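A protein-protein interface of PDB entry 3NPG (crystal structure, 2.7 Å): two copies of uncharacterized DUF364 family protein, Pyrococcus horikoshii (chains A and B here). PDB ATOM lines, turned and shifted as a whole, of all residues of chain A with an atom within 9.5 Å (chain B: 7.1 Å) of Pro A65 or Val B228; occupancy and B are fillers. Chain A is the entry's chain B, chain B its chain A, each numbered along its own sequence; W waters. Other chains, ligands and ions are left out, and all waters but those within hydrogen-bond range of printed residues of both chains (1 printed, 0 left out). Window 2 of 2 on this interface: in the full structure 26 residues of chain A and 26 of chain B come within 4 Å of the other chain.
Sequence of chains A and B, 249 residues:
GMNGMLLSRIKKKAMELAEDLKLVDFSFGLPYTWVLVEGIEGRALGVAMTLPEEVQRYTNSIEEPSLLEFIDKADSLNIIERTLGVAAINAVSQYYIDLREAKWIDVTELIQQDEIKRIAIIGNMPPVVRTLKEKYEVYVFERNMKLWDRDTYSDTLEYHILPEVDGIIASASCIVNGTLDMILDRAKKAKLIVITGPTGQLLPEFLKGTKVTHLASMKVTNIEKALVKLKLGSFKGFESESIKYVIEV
Among the printed residues, merely in contact across the chains: Phe A26 with Lys B231 (3.4 Å), Phe A26 with Leu B232 (3.6 Å), Ser A27 with Lys B231 (3.7 Å), Ile A62 with Leu B232 (3.5 Å), Pro A65 with Val B228 (3.8 Å), Phe A70 with Leu B232 (3.7 Å), Ile A80 with Leu B232 (3.1 Å), Ile A80 with Gly B233 (3.6 Å) and Leu A84 with Leu B232 (3.9 Å).
No position is printed for both chains.
Hydrophobic or aromatic side chains of chain A within 4 Å of the printed part of chain B: Phe A26, Phe A28, Pro A65, Phe A70, Ile A80 and Leu A84.
Along chain A the printed residues that touch a printed residue of chain B span positions 25 to 84.
Of the 13 printed residues of chain B, 5 touch a printed residue of chain A.
Hydrophobic or aromatic side chains of chain B that line the printed part of chain A: Val B228 and Leu B232.
Along chain B the printed residues that touch a printed residue of chain A span positions 228 to 233.
Among the printed residues, 13 pairs touch across the chains.
OE1 of Glu A63 is in salt-bridge range of NZ of Lys B229, at 2.8 Å.
The backbone carbonyl oxygen (O) of Lys B231 is in hydrogen-bond range of the backbone NH (N) of Phe A28, 2.8 Å away.
OD1 of Asp A25 is in salt-bridge range of NZ of Lys B231, 3.5 Å away.
ND2 of Asn A60 lies within hydrogen-bond range of O of Leu B232 (2.8 Å).
Water W1 lies within hydrogen-bond range of O of Asn A60 (2.5 Å), O of Ile A62 (2.7 Å) and NZ of Lys B229 (3.1 Å).
Printed residues of chain B within 4 Å of Phe A26: Lys B231 (3.4 Å) and Leu B232 (3.6 Å).
Printed residues of chain B within 4 Å of Phe A28: Lys B231.
Of chain B, only Val B228 (3.8 Å) comes within 4 Å of Pro A65.
Ile B223 touches none of the printed residues of chain A.
Of chain A, only Pro A65 comes within 4 Å of Val B228.
Printed residues of chain A within 4 Å of Lys B229: Glu A63 (2.8 Å).
Leu B230 touches none of the printed residues of chain A.
Printed residues of chain A within 4 Å of Leu B232: Phe A26, Asn A60, Ile A62, Phe A70, Ile A80 and Leu A84.
Printed residues of chain A within 4 Å of Gly B233: Ile A80 (3.6 Å).
The nearest residue of chain B that does not touch Pro A65 is Leu B232 (4.05 Å).
The nearest residue of chain A that does not touch Val B228 is Phe A26 (4.1 Å).
The nearest printed residue of chain B that does not touch Asp A25 is Leu B227 (7.3 Å).
N of Ile A62 is in hydrogen-bond range of OD1 of Asn A60, 3.1 Å away.
The backbone carbonyl oxygen of Lys B229 lies within hydrogen-bond range of the backbone NH of Ser B234 (2.9 Å).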
ATOM      1  N   LYS A  22     -14.708   0.723  -0.804  1.00  0.00           N
ATOM      2  CA  LYS A  22     -14.094   0.091  -1.978  1.00  0.00           C
ATOM      3  C   LYS A  22     -15.133  -0.637  -2.828  1.00  0.00           C
ATOM      4  O   LYS A  22     -16.122  -1.146  -2.296  1.00  0.00           O
ATOM      5  CB  LYS A  22     -12.953  -0.868  -1.563  1.00  0.00           C
ATOM      6  CG  LYS A  22     -13.403  -2.077  -0.732  1.00  0.00           C
ATOM      7  CD  LYS A  22     -12.217  -2.868  -0.197  1.00  0.00           C
ATOM      8  CE  LYS A  22     -12.657  -4.063   0.609  1.00  0.00           C
ATOM      9  N   LEU A  23     -14.901  -0.703  -4.148  1.00  0.00           N
ATOM     10  CA  LEU A  23     -15.794  -1.403  -5.067  1.00  0.00           C
ATOM     11  C   LEU A  23     -15.588  -2.919  -4.968  1.00  0.00           C
ATOM     12  O   LEU A  23     -14.454  -3.392  -5.036  1.00  0.00           O
ATOM     13  CB  LEU A  23     -15.552  -0.917  -6.515  1.00  0.00           C
ATOM     14  CG  LEU A  23     -16.363  -1.620  -7.625  1.00  0.00           C
ATOM     15  CD1 LEU A  23     -17.840  -1.278  -7.533  1.00  0.00           C
ATOM     16  CD2 LEU A  23     -15.835  -1.254  -8.996  1.00  0.00           C
ATOM     17  N   VAL A  24     -16.681  -3.674  -4.773  1.00  0.00           N
ATOM     18  CA  VAL A  24     -16.621  -5.140  -4.709  1.00  0.00           C
ATOM     19  C   VAL A  24     -17.030  -5.739  -6.064  1.00  0.00           C
ATOM     20  O   VAL A  24     -16.255  -6.470  -6.675  1.00  0.00           O
ATOM     21  CB  VAL A  24     -17.488  -5.707  -3.548  1.00  0.00           C
ATOM     22  CG1 VAL A  24     -17.508  -7.231  -3.577  1.00  0.00           C
ATOM     23  CG2 VAL A  24     -16.998  -5.199  -2.201  1.00  0.00           C
ATOM     24  N   ASP A  25     -18.254  -5.422  -6.522  1.00  0.00           N
ATOM     25  CA  ASP A  25     -18.790  -5.914  -7.788  1.00  0.00           C
ATOM     26  C   ASP A  25     -19.795  -4.898  -8.363  1.00  0.00           C
ATOM     27  O   ASP A  25     -20.237  -3.994  -7.648  1.00  0.00           O
ATOM     28  CB  ASP A  25     -19.461  -7.299  -7.595  1.00  0.00           C
ATOM     29  CG  ASP A  25     -19.502  -8.168  -8.852  1.00  0.00           C
ATOM     30  OD1 ASP A  25     -18.865  -7.784  -9.867  1.00  0.00           O
ATOM     31  OD2 ASP A  25     -20.127  -9.246  -8.804  1.00  0.00           O
ATOM     32  N   PHE A  26     -20.122  -5.026  -9.660  1.00  0.00           N
ATOM     33  CA  PHE A  26     -21.067  -4.139 -10.343  1.00  0.00           C
ATOM     34  C   PHE A  26     -21.652  -4.835 -11.574  1.00  0.00           C
ATOM     35  O   PHE A  26     -21.125  -5.865 -12.008  1.00  0.00           O
ATOM     36  CB  PHE A  26     -20.377  -2.815 -10.755  1.00  0.00           C
ATOM     37  CG  PHE A  26     -19.256  -2.990 -11.756  1.00  0.00           C
ATOM     38  CD1 PHE A  26     -17.967  -3.299 -11.335  1.00  0.00           C
ATOM     39  CD2 PHE A  26     -19.489  -2.850 -13.118  1.00  0.00           C
ATOM     40  CE1 PHE A  26     -16.938  -3.486 -12.261  1.00  0.00           C
ATOM     41  CE2 PHE A  26     -18.459  -3.030 -14.041  1.00  0.00           C
ATOM     42  CZ  PHE A  26     -17.189  -3.347 -13.606  1.00  0.00           C
ATOM     43  N   SER A  27     -22.720  -4.254 -12.162  1.00  0.00           N
ATOM     44  CA  SER A  27     -23.345  -4.797 -13.368  1.00  0.00           C
ATOM     45  C   SER A  27     -24.337  -3.822 -13.963  1.00  0.00           C
ATOM     46  O   SER A  27     -25.295  -3.429 -13.294  1.00  0.00           O
ATOM     47  CB  SER A  27     -24.042  -6.128 -13.072  1.00  0.00           C
ATOM     48  OG  SER A  27     -24.662  -6.666 -14.231  1.00  0.00           O
ATOM     49  N   PHE A  28     -24.140  -3.459 -15.240  1.00  0.00           N
ATOM     50  CA  PHE A  28     -25.109  -2.664 -15.978  1.00  0.00           C
ATOM     51  C   PHE A  28     -26.160  -3.628 -16.534  1.00  0.00           C
ATOM     52  O   PHE A  28     -25.990  -4.167 -17.630  1.00  0.00           O
ATOM     53  CB  PHE A  28     -24.415  -1.872 -17.114  1.00  0.00           C
ATOM     54  CG  PHE A  28     -25.350  -1.018 -17.942  1.00  0.00           C
ATOM     55  CD1 PHE A  28     -25.873   0.166 -17.432  1.00  0.00           C
ATOM     56  CD2 PHE A  28     -25.677  -1.379 -19.247  1.00  0.00           C
ATOM     57  CE1 PHE A  28     -26.749   0.947 -18.192  1.00  0.00           C
ATOM     58  CE2 PHE A  28     -26.543  -0.591 -20.011  1.00  0.00           C
ATOM     59  CZ  PHE A  28     -27.070   0.568 -19.481  1.00  0.00           C
ATOM     60  N   VAL A  35     -24.339  -1.601  -7.872  1.00  0.00           N
ATOM     61  CA  VAL A  35     -22.947  -1.461  -7.456  1.00  0.00           C
ATOM     62  C   VAL A  35     -22.817  -1.948  -6.013  1.00  0.00           C
ATOM     63  O   VAL A  35     -23.511  -1.440  -5.122  1.00  0.00           O
ATOM     64  CB  VAL A  35     -22.441   0.009  -7.617  1.00  0.00           C
ATOM     65  CG1 VAL A  35     -21.141   0.242  -6.850  1.00  0.00           C
ATOM     66  CG2 VAL A  35     -22.276   0.375  -9.088  1.00  0.00           C
ATOM     67  N   ASN A  60     -18.241   2.249 -23.024  1.00  0.00           N
ATOM     68  CA  ASN A  60     -17.894   2.761 -21.700  1.00  0.00           C
ATOM     69  C   ASN A  60     -16.420   3.187 -21.667  1.00  0.00           C
ATOM     70  O   ASN A  60     -15.539   2.385 -21.976  1.00  0.00           O
ATOM     71  CB  ASN A  60     -18.183   1.713 -20.622  1.00  0.00           C
ATOM     72  CG  ASN A  60     -18.439   2.299 -19.249  1.00  0.00           C
ATOM     73  OD1 ASN A  60     -17.703   3.156 -18.767  1.00  0.00           O
ATOM     74  ND2 ASN A  60     -19.453   1.788 -18.566  1.00  0.00           N
ATOM     75  N   SER A  61     -16.158   4.459 -21.320  1.00  0.00           N
ATOM     76  CA  SER A  61     -14.795   5.005 -21.266  1.00  0.00           C
ATOM     77  C   SER A  61     -14.001   4.473 -20.065  1.00  0.00           C
ATOM     78  O   SER A  61     -12.768   4.545 -20.066  1.00  0.00           O
ATOM     79  CB  SER A  61     -14.831   6.528 -21.242  1.00  0.00           C
ATOM     80  OG  SER A  61     -15.562   7.012 -20.129  1.00  0.00           O
ATOM     81  N   ILE A  62     -14.708   3.937 -19.036  1.00  0.00           N
ATOM     82  CA  ILE A  62     -14.066   3.379 -17.838  1.00  0.00           C
ATOM     83  C   ILE A  62     -13.241   2.131 -18.186  1.00  0.00           C
ATOM     84  O   ILE A  62     -13.796   1.130 -18.648  1.00  0.00           O
ATOM     85  CB  ILE A  62     -15.116   3.105 -16.716  1.00  0.00           C
ATOM     86  CG1 ILE A  62     -15.799   4.420 -16.258  1.00  0.00           C
ATOM     87  CG2 ILE A  62     -14.477   2.370 -15.532  1.00  0.00           C
ATOM     88  CD1 ILE A  62     -17.171   4.227 -15.570  1.00  0.00           C
ATOM     89  N   GLU A  63     -11.910   2.212 -17.999  1.00  0.00           N
ATOM     90  CA  GLU A  63     -11.011   1.087 -18.266  1.00  0.00           C
ATOM     91  C   GLU A  63     -10.720   0.321 -16.976  1.00  0.00           C
ATOM     92  O   GLU A  63     -10.833  -0.909 -16.948  1.00  0.00           O
ATOM     93  CB  GLU A  63      -9.704   1.570 -18.924  1.00  0.00           C
ATOM     94  CG  GLU A  63      -9.900   2.203 -20.299  1.00  0.00           C
ATOM     95  CD  GLU A  63     -10.518   1.299 -21.354  1.00  0.00           C
ATOM     96  OE1 GLU A  63     -10.141   0.106 -21.414  1.00  0.00           O
ATOM     97  OE2 GLU A  63     -11.353   1.797 -22.144  1.00  0.00           O
ATOM     98  N   GLU A  64     -10.380   1.053 -15.897  1.00  0.00           N
ATOM     99  CA  GLU A  64     -10.143   0.458 -14.586  1.00  0.00           C
ATOM    100  C   GLU A  64     -11.300   0.795 -13.641  1.00  0.00           C
ATOM    101  O   GLU A  64     -11.405   1.935 -13.170  1.00  0.00           O
ATOM    102  CB  GLU A  64      -8.800   0.935 -14.000  1.00  0.00           C
ATOM    103  CG  GLU A  64      -7.580   0.310 -14.667  1.00  0.00           C
ATOM    104  CD  GLU A  64      -7.401  -1.183 -14.438  1.00  0.00           C
ATOM    105  OE1 GLU A  64      -7.863  -1.690 -13.389  1.00  0.00           O
ATOM    106  OE2 GLU A  64      -6.751  -1.835 -15.286  1.00  0.00           O
ATOM    107  N   PRO A  65     -12.229  -0.162 -13.395  1.00  0.00           N
ATOM    108  CA  PRO A  65     -13.391   0.157 -12.551  1.00  0.00           C
ATOM    109  C   PRO A  65     -13.035   0.361 -11.085  1.00  0.00           C
ATOM    110  O   PRO A  65     -12.299  -0.437 -10.501  1.00  0.00           O
ATOM    111  CB  PRO A  65     -14.327  -1.052 -12.752  1.00  0.00           C
ATOM    112  CG  PRO A  65     -13.777  -1.789 -13.937  1.00  0.00           C
ATOM    113  CD  PRO A  65     -12.312  -1.532 -13.925  1.00  0.00           C
ATOM    114  N   SER A  66     -13.527   1.462 -10.503  1.00  0.00           N
ATOM    115  CA  SER A  66     -13.360   1.783  -9.088  1.00  0.00           C
ATOM    116  C   SER A  66     -14.559   2.598  -8.627  1.00  0.00           C
ATOM    117  O   SER A  66     -15.318   3.101  -9.463  1.00  0.00           O
ATOM    118  CB  SER A  66     -12.062   2.559  -8.853  1.00  0.00           C
ATOM    119  OG  SER A  66     -12.184   3.922  -9.227  1.00  0.00           O
ATOM    120  N   LEU A  67     -14.746   2.726  -7.307  1.00  0.00           N
ATOM    121  CA  LEU A  67     -15.870   3.471  -6.756  1.00  0.00           C
ATOM    122  C   LEU A  67     -15.807   4.964  -7.122  1.00  0.00           C
ATOM    123  O   LEU A  67     -16.810   5.521  -7.567  1.00  0.00           O
ATOM    124  CB  LEU A  67     -15.946   3.279  -5.236  1.00  0.00           C
ATOM    125  CG  LEU A  67     -17.172   3.869  -4.531  1.00  0.00           C
ATOM    126  CD1 LEU A  67     -18.478   3.427  -5.208  1.00  0.00           C
ATOM    127  CD2 LEU A  67     -17.183   3.486  -3.092  1.00  0.00           C
ATOM    128  N   LEU A  68     -14.615   5.591  -6.993  1.00  0.00           N
ATOM    129  CA  LEU A  68     -14.431   7.011  -7.326  1.00  0.00           C
ATOM    130  C   LEU A  68     -14.583   7.275  -8.834  1.00  0.00           C
ATOM    131  O   LEU A  68     -15.127   8.310  -9.219  1.00  0.00           O
ATOM    132  CB  LEU A  68     -13.065   7.521  -6.821  1.00  0.00           C
ATOM    133  CG  LEU A  68     -12.917   7.641  -5.291  1.00  0.00           C
ATOM    134  CD1 LEU A  68     -11.474   7.866  -4.904  1.00  0.00           C
ATOM    135  CD2 LEU A  68     -13.797   8.763  -4.730  1.00  0.00           C
ATOM    136  N   GLU A  69     -14.125   6.321  -9.685  1.00  0.00           N
ATOM    137  CA  GLU A  69     -14.244   6.424 -11.146  1.00  0.00           C
ATOM    138  C   GLU A  69     -15.723   6.364 -11.569  1.00  0.00           C
ATOM    139  O   GLU A  69     -16.152   7.150 -12.419  1.00  0.00           O
ATOM    140  CB  GLU A  69     -13.435   5.302 -11.836  1.00  0.00           C
ATOM    141  CG  GLU A  69     -13.430   5.375 -13.362  1.00  0.00           C
ATOM    142  CD  GLU A  69     -12.511   6.421 -13.970  1.00  0.00           C
ATOM    143  OE1 GLU A  69     -11.477   6.745 -13.342  1.00  0.00           O
ATOM    144  OE2 GLU A  69     -12.777   6.841 -15.119  1.00  0.00           O
ATOM    145  N   PHE A  70     -16.506   5.451 -10.951  1.00  0.00           N
ATOM    146  CA  PHE A  70     -17.937   5.313 -11.240  1.00  0.00           C
ATOM    147  C   PHE A  70     -18.692   6.584 -10.887  1.00  0.00           C
ATOM    148  O   PHE A  70     -19.424   7.112 -11.728  1.00  0.00           O
ATOM    149  CB  PHE A  70     -18.539   4.110 -10.487  1.00  0.00           C
ATOM    150  CG  PHE A  70     -18.295   2.749 -11.115  1.00  0.00           C
ATOM    151  CD1 PHE A  70     -17.641   2.633 -12.336  1.00  0.00           C
ATOM    152  CD2 PHE A  70     -18.754   1.592 -10.503  1.00  0.00           C
ATOM    153  CE1 PHE A  70     -17.419   1.379 -12.912  1.00  0.00           C
ATOM    154  CE2 PHE A  70     -18.534   0.340 -11.082  1.00  0.00           C
ATOM    155  CZ  PHE A  70     -17.865   0.242 -12.280  1.00  0.00           C
ATOM    156  N   ILE A  71     -18.473   7.116  -9.647  1.00  0.00           N
ATOM    157  CA  ILE A  71     -19.139   8.341  -9.171  1.00  0.00           C
ATOM    158  C   ILE A  71     -18.781   9.569 -10.035  1.00  0.00           C
ATOM    159  O   ILE A  71     -19.645  10.412 -10.276  1.00  0.00           O
ATOM    160  CB  ILE A  71     -18.871   8.588  -7.650  1.00  0.00           C
ATOM    161  CG1 ILE A  71     -19.290   7.364  -6.809  1.00  0.00           C
ATOM    162  CG2 ILE A  71     -19.589   9.862  -7.160  1.00  0.00           C
ATOM    163  CD1 ILE A  71     -18.756   7.365  -5.379  1.00  0.00           C
ATOM    164  N   LYS A  73     -18.303   9.678 -13.234  1.00  0.00           N
ATOM    165  CA  LYS A  73     -19.002   9.616 -14.526  1.00  0.00           C
ATOM    166  C   LYS A  73     -20.548   9.716 -14.352  1.00  0.00           C
ATOM    167  O   LYS A  73     -21.291   9.454 -15.302  1.00  0.00           O
ATOM    168  CB  LYS A  73     -18.628   8.316 -15.294  1.00  0.00           C
ATOM    169  CG  LYS A  73     -17.116   8.101 -15.495  1.00  0.00           C
ATOM    170  CD  LYS A  73     -16.555   8.903 -16.669  1.00  0.00           C
ATOM    171  CE  LYS A  73     -15.092   8.608 -16.894  1.00  0.00           C
ATOM    172  NZ  LYS A  73     -14.517   9.440 -17.985  1.00  0.00           N
ATOM    173  N   ILE A  80     -25.002   4.774 -19.863  1.00  0.00           N
ATOM    174  CA  ILE A  80     -24.378   3.615 -19.202  1.00  0.00           C
ATOM    175  C   ILE A  80     -23.460   4.087 -18.065  1.00  0.00           C
ATOM    176  O   ILE A  80     -23.524   3.548 -16.957  1.00  0.00           O
ATOM    177  CB  ILE A  80     -23.613   2.709 -20.223  1.00  0.00           C
ATOM    178  CG1 ILE A  80     -24.525   2.297 -21.408  1.00  0.00           C
ATOM    179  CG2 ILE A  80     -23.019   1.489 -19.525  1.00  0.00           C
ATOM    180  CD1 ILE A  80     -23.808   1.610 -22.535  1.00  0.00           C
ATOM    181  N   LEU A  84     -24.363   3.609 -13.912  1.00  0.00           N
ATOM    182  CA  LEU A  84     -23.341   2.996 -13.046  1.00  0.00           C
ATOM    183  C   LEU A  84     -22.861   3.984 -11.970  1.00  0.00           C
ATOM    184  O   LEU A  84     -22.564   3.575 -10.849  1.00  0.00           O
ATOM    185  CB  LEU A  84     -22.149   2.494 -13.883  1.00  0.00           C
ATOM    186  CG  LEU A  84     -22.339   1.140 -14.582  1.00  0.00           C
ATOM    187  CD1 LEU A  84     -21.390   0.995 -15.749  1.00  0.00           C
ATOM    188  CD2 LEU A  84     -22.145   0.000 -13.620  1.00  0.00           C
ATOM    189  N   ASN B 222     -10.090 -14.188 -22.901  1.00  0.00           N
ATOM    190  CA  ASN B 222      -9.809 -13.749 -21.532  1.00  0.00           C
ATOM    191  C   ASN B 222     -11.132 -13.513 -20.810  1.00  0.00           C
ATOM    192  O   ASN B 222     -11.790 -12.496 -21.037  1.00  0.00           O
ATOM    193  CB  ASN B 222      -8.945 -12.469 -21.529  1.00  0.00           C
ATOM    194  CG  ASN B 222      -8.321 -12.137 -20.183  1.00  0.00           C
ATOM    195  OD1 ASN B 222      -8.967 -12.192 -19.125  1.00  0.00           O
ATOM    196  ND2 ASN B 222      -7.071 -11.715 -20.208  1.00  0.00           N
ATOM    197  N   ILE B 223     -11.557 -14.490 -19.995  1.00  0.00           N
ATOM    198  CA  ILE B 223     -12.840 -14.446 -19.278  1.00  0.00           C
ATOM    199  C   ILE B 223     -12.930 -13.244 -18.314  1.00  0.00           C
ATOM    200  O   ILE B 223     -13.951 -12.553 -18.294  1.00  0.00           O
ATOM    201  CB  ILE B 223     -13.111 -15.796 -18.547  1.00  0.00           C
ATOM    202  CG1 ILE B 223     -12.925 -17.025 -19.501  1.00  0.00           C
ATOM    203  CG2 ILE B 223     -14.473 -15.794 -17.850  1.00  0.00           C
ATOM    204  CD1 ILE B 223     -14.038 -17.279 -20.530  1.00  0.00           C
ATOM    205  N   GLU B 224     -11.865 -13.004 -17.518  1.00  0.00           N
ATOM    206  CA  GLU B 224     -11.850 -11.921 -16.528  1.00  0.00           C
ATOM    207  C   GLU B 224     -11.997 -10.539 -17.170  1.00  0.00           C
ATOM    208  O   GLU B 224     -12.826  -9.744 -16.722  1.00  0.00           O
ATOM    209  CB  GLU B 224     -10.582 -11.988 -15.655  1.00  0.00           C
ATOM    210  CG  GLU B 224     -10.568 -13.165 -14.688  1.00  0.00           C
ATOM    211  CD  GLU B 224     -11.667 -13.150 -13.638  1.00  0.00           C
ATOM    212  OE1 GLU B 224     -11.946 -12.064 -13.078  1.00  0.00           O
ATOM    213  OE2 GLU B 224     -12.234 -14.232 -13.360  1.00  0.00           O
ATOM    214  N   LYS B 225     -11.209 -10.259 -18.230  1.00  0.00           N
ATOM    215  CA  LYS B 225     -11.253  -8.964 -18.923  1.00  0.00           C
ATOM    216  C   LYS B 225     -12.582  -8.758 -19.669  1.00  0.00           C
ATOM    217  O   LYS B 225     -13.108  -7.642 -19.686  1.00  0.00           O
ATOM    218  CB  LYS B 225     -10.062  -8.810 -19.877  1.00  0.00           C
ATOM    219  CG  LYS B 225      -8.730  -8.609 -19.169  1.00  0.00           C
ATOM    220  CD  LYS B 225      -7.668  -8.086 -20.127  1.00  0.00           C
ATOM    221  CE  LYS B 225      -6.333  -7.900 -19.451  1.00  0.00           C
ATOM    222  NZ  LYS B 225      -5.350  -7.241 -20.352  1.00  0.00           N
ATOM    223  N   ALA B 226     -13.137  -9.845 -20.262  1.00  0.00           N
ATOM    224  CA  ALA B 226     -14.414  -9.794 -20.981  1.00  0.00           C
ATOM    225  C   ALA B 226     -15.597  -9.565 -20.024  1.00  0.00           C
ATOM    226  O   ALA B 226     -16.521  -8.836 -20.371  1.00  0.00           O
ATOM    227  CB  ALA B 226     -14.621 -11.068 -21.776  1.00  0.00           C
ATOM    228  N   LEU B 227     -15.550 -10.167 -18.804  1.00  0.00           N
ATOM    229  CA  LEU B 227     -16.590  -9.972 -17.776  1.00  0.00           C
ATOM    230  C   LEU B 227     -16.629  -8.533 -17.296  1.00  0.00           C
ATOM    231  O   LEU B 227     -17.708  -7.992 -17.066  1.00  0.00           O
ATOM    232  CB  LEU B 227     -16.365 -10.915 -16.579  1.00  0.00           C
ATOM    233  CG  LEU B 227     -16.933 -12.319 -16.720  1.00  0.00           C
ATOM    234  CD1 LEU B 227     -16.514 -13.182 -15.565  1.00  0.00           C
ATOM    235  CD2 LEU B 227     -18.438 -12.288 -16.828  1.00  0.00           C
ATOM    236  N   VAL B 228     -15.450  -7.902 -17.162  1.00  0.00           N
ATOM    237  CA  VAL B 228     -15.341  -6.496 -16.771  1.00  0.00           C
ATOM    238  C   VAL B 228     -16.063  -5.614 -17.789  1.00  0.00           C
ATOM    239  O   VAL B 228     -16.856  -4.759 -17.405  1.00  0.00           O
ATOM    240  CB  VAL B 228     -13.850  -6.077 -16.579  1.00  0.00           C
ATOM    241  CG1 VAL B 228     -13.701  -4.559 -16.525  1.00  0.00           C
ATOM    242  CG2 VAL B 228     -13.259  -6.722 -15.330  1.00  0.00           C
ATOM    243  N   LYS B 229     -15.853  -5.880 -19.086  1.00  0.00           N
ATOM    244  CA  LYS B 229     -16.493  -5.110 -20.153  1.00  0.00           C
ATOM    245  C   LYS B 229     -17.986  -5.420 -20.265  1.00  0.00           C
ATOM    246  O   LYS B 229     -18.778  -4.504 -20.478  1.00  0.00           O
ATOM    247  CB  LYS B 229     -15.774  -5.331 -21.498  1.00  0.00           C
ATOM    248  CG  LYS B 229     -14.277  -4.954 -21.474  1.00  0.00           C
ATOM    249  CD  LYS B 229     -14.052  -3.438 -21.422  1.00  0.00           C
ATOM    250  CE  LYS B 229     -12.585  -3.094 -21.468  1.00  0.00           C
ATOM    251  NZ  LYS B 229     -12.353  -1.640 -21.271  1.00  0.00           N
ATOM    252  N   LEU B 230     -18.384  -6.711 -20.078  1.00  0.00           N
ATOM    253  CA  LEU B 230     -19.811  -7.097 -20.118  1.00  0.00           C
ATOM    254  C   LEU B 230     -20.581  -6.397 -19.004  1.00  0.00           C
ATOM    255  O   LEU B 230     -21.686  -5.894 -19.235  1.00  0.00           O
ATOM    256  CB  LEU B 230     -19.984  -8.626 -19.989  1.00  0.00           C
ATOM    257  CG  LEU B 230     -19.744  -9.458 -21.249  1.00  0.00           C
ATOM    258  CD1 LEU B 230     -19.738 -10.916 -20.924  1.00  0.00           C
ATOM    259  CD2 LEU B 230     -20.794  -9.177 -22.309  1.00  0.00           C
ATOM    260  N   LYS B 231     -19.976  -6.332 -17.795  1.00  0.00           N
ATOM    261  CA  LYS B 231     -20.567  -5.661 -16.634  1.00  0.00           C
ATOM    262  C   LYS B 231     -20.606  -4.143 -16.833  1.00  0.00           C
ATOM    263  O   LYS B 231     -21.499  -3.479 -16.302  1.00  0.00           O
ATOM    264  CB  LYS B 231     -19.793  -6.014 -15.355  1.00  0.00           C
ATOM    265  CG  LYS B 231     -20.050  -7.423 -14.851  1.00  0.00           C
ATOM    266  CD  LYS B 231     -18.971  -7.871 -13.883  1.00  0.00           C
ATOM    267  CE  LYS B 231     -19.344  -9.162 -13.212  1.00  0.00           C
ATOM    268  NZ  LYS B 231     -18.164  -9.845 -12.635  1.00  0.00           N
ATOM    269  N   LEU B 232     -19.643  -3.593 -17.616  1.00  0.00           N
ATOM    270  CA  LEU B 232     -19.578  -2.153 -17.905  1.00  0.00           C
ATOM    271  C   LEU B 232     -20.514  -1.749 -19.053  1.00  0.00           C
ATOM    272  O   LEU B 232     -20.725  -0.562 -19.282  1.00  0.00           O
ATOM    273  CB  LEU B 232     -18.130  -1.722 -18.223  1.00  0.00           C
ATOM    274  CG  LEU B 232     -17.216  -1.488 -17.018  1.00  0.00           C
ATOM    275  CD1 LEU B 232     -15.776  -1.458 -17.438  1.00  0.00           C
ATOM    276  CD2 LEU B 232     -17.582  -0.206 -16.291  1.00  0.00           C
ATOM    277  N   GLY B 233     -21.061  -2.740 -19.757  1.00  0.00           N
ATOM    278  CA  GLY B 233     -21.969  -2.509 -20.876  1.00  0.00           C
ATOM    279  C   GLY B 233     -21.256  -2.116 -22.156  1.00  0.00           C
ATOM    280  O   GLY B 233     -21.828  -1.416 -22.995  1.00  0.00           O
ATOM    281  N   SER B 234     -19.980  -2.547 -22.307  1.00  0.00           N
ATOM    282  CA  SER B 234     -19.163  -2.239 -23.485  1.00  0.00           C
ATOM    283  C   SER B 234     -19.066  -3.456 -24.393  1.00  0.00           C
ATOM    284  O   SER B 234     -18.480  -4.469 -24.000  1.00  0.00           O
ATOM    285  CB  SER B 234     -17.766  -1.788 -23.059  1.00  0.00           C
ATOM    286  OG  SER B 234     -16.959  -1.447 -24.175  1.00  0.00           O
HETATM  287  O   HOH W   1     -14.786   0.195 -20.950  1.00  0.00           O
